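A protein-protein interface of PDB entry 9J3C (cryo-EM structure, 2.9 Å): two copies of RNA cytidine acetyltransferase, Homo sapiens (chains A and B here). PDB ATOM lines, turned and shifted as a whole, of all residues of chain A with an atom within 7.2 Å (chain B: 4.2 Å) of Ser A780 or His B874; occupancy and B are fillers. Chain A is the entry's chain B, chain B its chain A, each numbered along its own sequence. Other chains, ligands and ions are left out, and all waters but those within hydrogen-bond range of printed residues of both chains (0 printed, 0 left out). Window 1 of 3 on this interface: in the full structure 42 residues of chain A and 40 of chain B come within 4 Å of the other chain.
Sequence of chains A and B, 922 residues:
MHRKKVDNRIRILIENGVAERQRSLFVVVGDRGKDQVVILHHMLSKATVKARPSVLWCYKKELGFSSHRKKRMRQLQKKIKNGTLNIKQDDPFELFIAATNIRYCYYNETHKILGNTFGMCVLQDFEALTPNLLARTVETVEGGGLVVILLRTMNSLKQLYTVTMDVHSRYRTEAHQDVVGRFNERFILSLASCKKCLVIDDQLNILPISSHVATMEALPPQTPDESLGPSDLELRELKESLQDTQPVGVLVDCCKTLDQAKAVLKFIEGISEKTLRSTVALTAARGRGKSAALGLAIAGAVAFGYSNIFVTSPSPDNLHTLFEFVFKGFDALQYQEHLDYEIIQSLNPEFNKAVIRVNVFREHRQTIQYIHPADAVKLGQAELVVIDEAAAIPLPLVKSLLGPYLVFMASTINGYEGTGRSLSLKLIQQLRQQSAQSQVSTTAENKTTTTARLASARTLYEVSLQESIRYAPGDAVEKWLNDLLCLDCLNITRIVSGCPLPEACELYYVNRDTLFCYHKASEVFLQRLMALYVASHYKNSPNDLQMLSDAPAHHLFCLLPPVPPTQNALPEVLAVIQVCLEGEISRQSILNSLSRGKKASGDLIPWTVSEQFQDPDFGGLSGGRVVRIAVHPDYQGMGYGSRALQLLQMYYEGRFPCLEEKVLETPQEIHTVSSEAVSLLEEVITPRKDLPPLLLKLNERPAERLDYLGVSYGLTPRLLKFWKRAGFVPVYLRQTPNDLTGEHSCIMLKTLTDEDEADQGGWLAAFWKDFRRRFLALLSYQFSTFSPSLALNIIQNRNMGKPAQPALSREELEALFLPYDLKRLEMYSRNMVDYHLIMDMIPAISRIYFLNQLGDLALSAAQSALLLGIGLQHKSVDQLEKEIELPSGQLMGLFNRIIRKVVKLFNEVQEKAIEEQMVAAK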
ATOM      1  N   PHE A 775       9.307  -4.602   5.487  1.00  0.00           N
ATOM      2  CA  PHE A 775       8.570  -4.993   4.290  1.00  0.00           C
ATOM      3  C   PHE A 775       9.077  -4.257   3.054  1.00  0.00           C
ATOM      4  O   PHE A 775       9.054  -4.806   1.947  1.00  0.00           O
ATOM      5  CB  PHE A 775       7.075  -4.740   4.488  1.00  0.00           C
ATOM      6  CG  PHE A 775       6.210  -5.373   3.435  1.00  0.00           C
ATOM      7  CD1 PHE A 775       5.977  -6.737   3.439  1.00  0.00           C
ATOM      8  CD2 PHE A 775       5.630  -4.601   2.442  1.00  0.00           C
ATOM      9  CE1 PHE A 775       5.181  -7.321   2.472  1.00  0.00           C
ATOM     10  CE2 PHE A 775       4.833  -5.179   1.473  1.00  0.00           C
ATOM     11  CZ  PHE A 775       4.609  -6.541   1.487  1.00  0.00           C
ATOM     12  N   LEU A 776       9.528  -3.012   3.222  1.00  0.00           N
ATOM     13  CA  LEU A 776      10.048  -2.257   2.086  1.00  0.00           C
ATOM     14  C   LEU A 776      11.290  -2.921   1.504  1.00  0.00           C
ATOM     15  O   LEU A 776      11.429  -3.031   0.280  1.00  0.00           O
ATOM     16  CB  LEU A 776      10.357  -0.820   2.509  1.00  0.00           C
ATOM     17  CG  LEU A 776       9.160   0.076   2.834  1.00  0.00           C
ATOM     18  CD1 LEU A 776       9.605   1.518   3.024  1.00  0.00           C
ATOM     19  CD2 LEU A 776       8.098  -0.023   1.751  1.00  0.00           C
ATOM     20  N   ALA A 777      12.205  -3.370   2.366  1.00  0.00           N
ATOM     21  CA  ALA A 777      13.412  -4.038   1.895  1.00  0.00           C
ATOM     22  C   ALA A 777      13.147  -5.478   1.473  1.00  0.00           C
ATOM     23  O   ALA A 777      13.867  -6.009   0.619  1.00  0.00           O
ATOM     24  CB  ALA A 777      14.491  -3.999   2.978  1.00  0.00           C
ATOM     25  N   LEU A 778      12.134  -6.122   2.051  1.00  0.00           N
ATOM     26  CA  LEU A 778      11.834  -7.513   1.740  1.00  0.00           C
ATOM     27  C   LEU A 778      10.945  -7.673   0.514  1.00  0.00           C
ATOM     28  O   LEU A 778      10.630  -8.809   0.143  1.00  0.00           O
ATOM     29  CB  LEU A 778      11.170  -8.190   2.942  1.00  0.00           C
ATOM     30  CG  LEU A 778      12.096  -8.540   4.109  1.00  0.00           C
ATOM     31  CD1 LEU A 778      11.309  -9.137   5.265  1.00  0.00           C
ATOM     32  CD2 LEU A 778      13.196  -9.484   3.654  1.00  0.00           C
ATOM     33  N   LEU A 779      10.537  -6.575  -0.119  1.00  0.00           N
ATOM     34  CA  LEU A 779       9.667  -6.638  -1.287  1.00  0.00           C
ATOM     35  C   LEU A 779      10.433  -7.092  -2.523  1.00  0.00           C
ATOM     36  O   LEU A 779       9.835  -7.337  -3.575  1.00  0.00           O
ATOM     37  CB  LEU A 779       9.014  -5.277  -1.540  1.00  0.00           C
ATOM     38  CG  LEU A 779       7.566  -5.108  -1.078  1.00  0.00           C
ATOM     39  CD1 LEU A 779       7.153  -3.646  -1.137  1.00  0.00           C
ATOM     40  CD2 LEU A 779       6.632  -5.962  -1.918  1.00  0.00           C
ATOM     41  N   SER A 780      11.757  -7.204  -2.410  1.00  0.00           N
ATOM     42  CA  SER A 780      12.603  -7.564  -3.539  1.00  0.00           C
ATOM     43  C   SER A 780      13.100  -9.002  -3.504  1.00  0.00           C
ATOM     44  O   SER A 780      13.649  -9.470  -4.507  1.00  0.00           O
ATOM     45  CB  SER A 780      13.812  -6.619  -3.615  1.00  0.00           C
ATOM     46  OG  SER A 780      13.397  -5.268  -3.727  1.00  0.00           O
ATOM     47  N   TYR A 781      12.927  -9.714  -2.390  1.00  0.00           N
ATOM     48  CA  TYR A 781      13.428 -11.082  -2.280  1.00  0.00           C
ATOM     49  C   TYR A 781      12.363 -12.109  -2.653  1.00  0.00           C
ATOM     50  O   TYR A 781      12.544 -12.889  -3.594  1.00  0.00           O
ATOM     51  CB  TYR A 781      13.945 -11.337  -0.859  1.00  0.00           C
ATOM     52  CG  TYR A 781      15.380 -10.918  -0.646  1.00  0.00           C
ATOM     53  CD1 TYR A 781      15.697  -9.613  -0.293  1.00  0.00           C
ATOM     54  CD2 TYR A 781      16.420 -11.825  -0.801  1.00  0.00           C
ATOM     55  CE1 TYR A 781      17.008  -9.225  -0.097  1.00  0.00           C
ATOM     56  CE2 TYR A 781      17.734 -11.446  -0.608  1.00  0.00           C
ATOM     57  CZ  TYR A 781      18.022 -10.145  -0.256  1.00  0.00           C
ATOM     58  OH  TYR A 781      19.329  -9.763  -0.063  1.00  0.00           O
ATOM     59  N   GLN A 782      11.247 -12.120  -1.926  1.00  0.00           N
ATOM     60  CA  GLN A 782      10.165 -13.061  -2.183  1.00  0.00           C
ATOM     61  C   GLN A 782       8.801 -12.411  -2.347  1.00  0.00           C
ATOM     62  O   GLN A 782       7.883 -13.075  -2.841  1.00  0.00           O
ATOM     63  CB  GLN A 782      10.079 -14.104  -1.057  1.00  0.00           C
ATOM     64  CG  GLN A 782      10.966 -15.319  -1.269  1.00  0.00           C
ATOM     65  CD  GLN A 782      11.781 -15.667  -0.040  1.00  0.00           C
ATOM     66  OE1 GLN A 782      12.326 -14.788   0.627  1.00  0.00           O
ATOM     67  NE2 GLN A 782      11.868 -16.957   0.267  1.00  0.00           N
ATOM     68  N   PHE A 783       8.634 -11.151  -1.957  1.00  0.00           N
ATOM     69  CA  PHE A 783       7.370 -10.446  -2.115  1.00  0.00           C
ATOM     70  C   PHE A 783       7.266  -9.717  -3.448  1.00  0.00           C
ATOM     71  O   PHE A 783       6.285  -8.999  -3.669  1.00  0.00           O
ATOM     72  CB  PHE A 783       7.173  -9.454  -0.964  1.00  0.00           C
ATOM     73  CG  PHE A 783       7.170 -10.095   0.394  1.00  0.00           C
ATOM     74  CD1 PHE A 783       6.564 -11.325   0.593  1.00  0.00           C
ATOM     75  CD2 PHE A 783       7.775  -9.470   1.471  1.00  0.00           C
ATOM     76  CE1 PHE A 783       6.560 -11.918   1.841  1.00  0.00           C
ATOM     77  CE2 PHE A 783       7.775 -10.059   2.722  1.00  0.00           C
ATOM     78  CZ  PHE A 783       7.166 -11.284   2.907  1.00  0.00           C
ATOM     79  N   SER A 784       8.255  -9.875  -4.332  1.00  0.00           N
ATOM     80  CA  SER A 784       8.182  -9.244  -5.646  1.00  0.00           C
ATOM     81  C   SER A 784       7.043  -9.811  -6.481  1.00  0.00           C
ATOM     82  O   SER A 784       6.485  -9.104  -7.326  1.00  0.00           O
ATOM     83  CB  SER A 784       9.512  -9.407  -6.380  1.00  0.00           C
ATOM     84  OG  SER A 784      10.061 -10.694  -6.162  1.00  0.00           O
ATOM     85  N   GLY A 871       9.998   0.620  -8.207  1.00  0.00           N
ATOM     86  CA  GLY A 871      11.079   0.843  -7.266  1.00  0.00           C
ATOM     87  C   GLY A 871      11.358  -0.310  -6.325  1.00  0.00           C
ATOM     88  O   GLY A 871      12.453  -0.880  -6.342  1.00  0.00           O
ATOM     89  N   LEU A 872      10.374  -0.662  -5.495  1.00  0.00           N
ATOM     90  CA  LEU A 872      10.599  -1.684  -4.479  1.00  0.00           C
ATOM     91  C   LEU A 872      10.639  -3.082  -5.086  1.00  0.00           C
ATOM     92  O   LEU A 872      11.491  -3.899  -4.718  1.00  0.00           O
ATOM     93  CB  LEU A 872       9.519  -1.597  -3.401  1.00  0.00           C
ATOM     94  CG  LEU A 872       9.466  -0.280  -2.626  1.00  0.00           C
ATOM     95  CD1 LEU A 872       8.132  -0.132  -1.915  1.00  0.00           C
ATOM     96  CD2 LEU A 872      10.618  -0.193  -1.636  1.00  0.00           C
ATOM     97  N   GLN A 873       9.728  -3.377  -6.011  1.00  0.00           N
ATOM     98  CA  GLN A 873       9.645  -4.704  -6.606  1.00  0.00           C
ATOM     99  C   GLN A 873      10.530  -4.872  -7.833  1.00  0.00           C
ATOM    100  O   GLN A 873      10.671  -5.999  -8.320  1.00  0.00           O
ATOM    101  CB  GLN A 873       8.193  -5.024  -6.977  1.00  0.00           C
ATOM    102  CG  GLN A 873       7.352  -5.525  -5.814  1.00  0.00           C
ATOM    103  CD  GLN A 873       5.896  -5.721  -6.188  1.00  0.00           C
ATOM    104  OE1 GLN A 873       5.373  -5.041  -7.070  1.00  0.00           O
ATOM    105  NE2 GLN A 873       5.234  -6.655  -5.516  1.00  0.00           N
ATOM    106  N   HIS A 874      11.129  -3.788  -8.332  1.00  0.00           N
ATOM    107  CA  HIS A 874      11.997  -3.831  -9.511  1.00  0.00           C
ATOM    108  C   HIS A 874      11.282  -4.462 -10.703  1.00  0.00           C
ATOM    109  O   HIS A 874      11.861  -5.242 -11.463  1.00  0.00           O
ATOM    110  CB  HIS A 874      13.305  -4.564  -9.206  1.00  0.00           C
ATOM    111  CG  HIS A 874      13.890  -4.225  -7.870  1.00  0.00           C
ATOM    112  ND1 HIS A 874      14.330  -2.960  -7.550  1.00  0.00           N
ATOM    113  CD2 HIS A 874      14.109  -4.988  -6.774  1.00  0.00           C
ATOM    114  CE1 HIS A 874      14.795  -2.956  -6.313  1.00  0.00           C
ATOM    115  NE2 HIS A 874      14.672  -4.175  -5.819  1.00  0.00           N
ATOM    116  N   SER B 780      19.546  -4.726 -10.023  1.00  0.00           N
ATOM    117  CA  SER B 780      18.284  -5.330  -9.625  1.00  0.00           C
ATOM    118  C   SER B 780      17.195  -5.237 -10.686  1.00  0.00           C
ATOM    119  O   SER B 780      16.153  -5.883 -10.532  1.00  0.00           O
ATOM    120  CB  SER B 780      17.773  -4.684  -8.328  1.00  0.00           C
ATOM    121  OG  SER B 780      18.735  -4.794  -7.293  1.00  0.00           O
ATOM    122  N   GLY B 869      25.435 -11.282  -5.024  1.00  0.00           N
ATOM    123  CA  GLY B 869      24.253 -11.954  -5.538  1.00  0.00           C
ATOM    124  C   GLY B 869      23.056 -11.851  -4.611  1.00  0.00           C
ATOM    125  O   GLY B 869      21.937 -11.584  -5.057  1.00  0.00           O
ATOM    126  N   ILE B 870      23.271 -12.067  -3.313  1.00  0.00           N
ATOM    127  CA  ILE B 870      22.164 -12.036  -2.362  1.00  0.00           C
ATOM    128  C   ILE B 870      21.658 -10.611  -2.174  1.00  0.00           C
ATOM    129  O   ILE B 870      20.447 -10.359  -2.175  1.00  0.00           O
ATOM    130  CB  ILE B 870      22.588 -12.666  -1.023  1.00  0.00           C
ATOM    131  CG1 ILE B 870      22.974 -14.133  -1.223  1.00  0.00           C
ATOM    132  CG2 ILE B 870      21.471 -12.545   0.002  1.00  0.00           C
ATOM    133  CD1 ILE B 870      23.294 -14.862   0.065  1.00  0.00           C
ATOM    134  N   GLY B 871      22.573  -9.658  -2.014  1.00  0.00           N
ATOM    135  CA  GLY B 871      22.188  -8.292  -1.722  1.00  0.00           C
ATOM    136  C   GLY B 871      21.763  -7.475  -2.925  1.00  0.00           C
ATOM    137  O   GLY B 871      20.618  -7.017  -2.998  1.00  0.00           O
ATOM    138  N   LEU B 872      22.678  -7.281  -3.875  1.00  0.00           N
ATOM    139  CA  LEU B 872      22.388  -6.409  -5.010  1.00  0.00           C
ATOM    140  C   LEU B 872      21.442  -7.073  -6.003  1.00  0.00           C
ATOM    141  O   LEU B 872      20.522  -6.428  -6.518  1.00  0.00           O
ATOM    142  CB  LEU B 872      23.689  -5.997  -5.698  1.00  0.00           C
ATOM    143  CG  LEU B 872      24.662  -5.192  -4.837  1.00  0.00           C
ATOM    144  CD1 LEU B 872      26.058  -5.225  -5.434  1.00  0.00           C
ATOM    145  CD2 LEU B 872      24.179  -3.759  -4.674  1.00  0.00           C
ATOM    146  N   GLN B 873      21.649  -8.358  -6.286  1.00  0.00           N
ATOM    147  CA  GLN B 873      20.835  -9.066  -7.263  1.00  0.00           C
ATOM    148  C   GLN B 873      19.589  -9.703  -6.662  1.00  0.00           C
ATOM    149  O   GLN B 873      18.746 -10.201  -7.419  1.00  0.00           O
ATOM    150  CB  GLN B 873      21.670 -10.143  -7.965  1.00  0.00           C
ATOM    151  CG  GLN B 873      22.519  -9.618  -9.111  1.00  0.00           C
ATOM    152  CD  GLN B 873      23.422 -10.682  -9.704  1.00  0.00           C
ATOM    153  OE1 GLN B 873      23.816 -11.628  -9.022  1.00  0.00           O
ATOM    154  NE2 GLN B 873      23.754 -10.532 -10.981  1.00  0.00           N
ATOM    155  N   HIS B 874      19.452  -9.692  -5.335  1.00  0.00           N
ATOM    156  CA  HIS B 874      18.294 -10.271  -4.649  1.00  0.00           C
ATOM    157  C   HIS B 874      18.084 -11.729  -5.048  1.00  0.00           C
ATOM    158  O   HIS B 874      16.958 -12.183  -5.264  1.00  0.00           O
ATOM    159  CB  HIS B 874      17.032  -9.446  -4.907  1.00  0.00           C
ATOM    160  CG  HIS B 874      17.250  -7.967  -4.827  1.00  0.00           C
ATOM    161  ND1 HIS B 874      17.671  -7.338  -3.674  1.00  0.00           N
ATOM    162  CD2 HIS B 874      17.104  -6.992  -5.755  1.00  0.00           C
ATOM    163  CE1 HIS B 874      17.775  -6.040  -3.897  1.00  0.00           C
ATOM    164  NE2 HIS B 874      17.438  -5.804  -5.152  1.00  0.00           N
ATOM    165  N   LYS B 875      19.183 -12.472  -5.149  1.00  0.00           N
ATOM    166  CA  LYS B 875      19.137 -13.874  -5.534  1.00  0.00           C
ATOM    167  C   LYS B 875      18.997 -14.759  -4.304  1.00  0.00           C
ATOM    168  O   LYS B 875      19.636 -14.521  -3.275  1.00  0.00           O
ATOM    169  CB  LYS B 875      20.394 -14.263  -6.313  1.00  0.00           C
ATOM    170  CG  LYS B 875      20.388 -13.832  -7.768  1.00  0.00           C
ATOM    171  CD  LYS B 875      21.708 -14.167  -8.439  1.00  0.00           C
ATOM    172  CE  LYS B 875      21.587 -14.134  -9.953  1.00  0.00           C
ATOM    173  NZ  LYS B 875      20.177 -13.960 -10.399  1.00  0.00           N
ATOM    174  N   SER B 876      18.156 -15.783  -4.418  1.00  0.00           N
ATOM    175  CA  SER B 876      17.987 -16.735  -3.334  1.00  0.00           C
ATOM    176  C   SER B 876      19.210 -17.640  -3.224  1.00  0.00           C
ATOM    177  O   SER B 876      20.023 -17.754  -4.147  1.00  0.00           O
ATOM    178  CB  SER B 876      16.726 -17.573  -3.545  1.00  0.00           C
ATOM    179  OG  SER B 876      16.660 -18.072  -4.868  1.00  0.00           O
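NE2 of His A874 is in hydrogen-bond range of NE2 of His B874, at 3.3 Å. The side-chain hydroxyl of Tyr A781 sits at hydrogen-bond distance from the backbone carbonyl oxygen of Ile B870 (2.5 Å).
The backbone carbonyl oxygen (O) of Leu A872 is in hydrogen-bond range of the side-chain hydroxyl (OG) of Ser A780, 2.5 Å away. NE2 of His B874 lies within hydrogen-bond range of OG of Ser B780. NE2 of His A874 sits at hydrogen-bond distance from OG of Ser A780, at 2.7 Å. O of Leu A872 is in hydrogen-bond range of NE2 of His A874, at 3.4 Å. ND1 of His A874 is in hydrogen-bond range of O of Gly A871 (3.1 Å). O of Gly B869 sits at hydrogen-bond distance from N of His B874 (3.1 Å).
Of the 14 printed residues of chain A, 3 touch a printed residue of chain B. Hydrophobic or aromatic side chains of chain A that line the printed part of chain B: Tyr A781 and His A874. Hydrophobic or aromatic side chains of chain B within 4 Å of the printed part of chain A: Ile B870 and His B874. Among the printed residues, 5 pairs touch across the chains. Among the printed residues, no Asp or Glu carboxylate lies within 4 Å of a Lys or Arg side-chain nitrogen of the other chain.
Ser A780 touches His B874, and with the chains exchanged His A874 touches Ser B780. His A874 touches its own counterpart, His B874. Of the 5 pairs that touch across the chains among the printed residues, 3 have their exchanged pair printed and touching as well.
Among the printed residues, pairs that only touch across the chains: Ser A780 with His B874, Tyr A781 with Gly B871 and His A874 with Ser B780.
Ser A780 touches one residue of chain B. Of the printed residues of chain B, His A874 touches Ser B780 and His B874. Of the printed residues of chain A, Ile B870 touches Tyr A781. Of the printed residues of chain A, Gly B871 touches Tyr A781. Printed residues of chain A within 4 Å of His B874: Ser A780 (3.4 Å) and His A874 (3.3 Å). The nearest residue of chain A that does not touch His B874 is Tyr A781 (4.1 Å).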
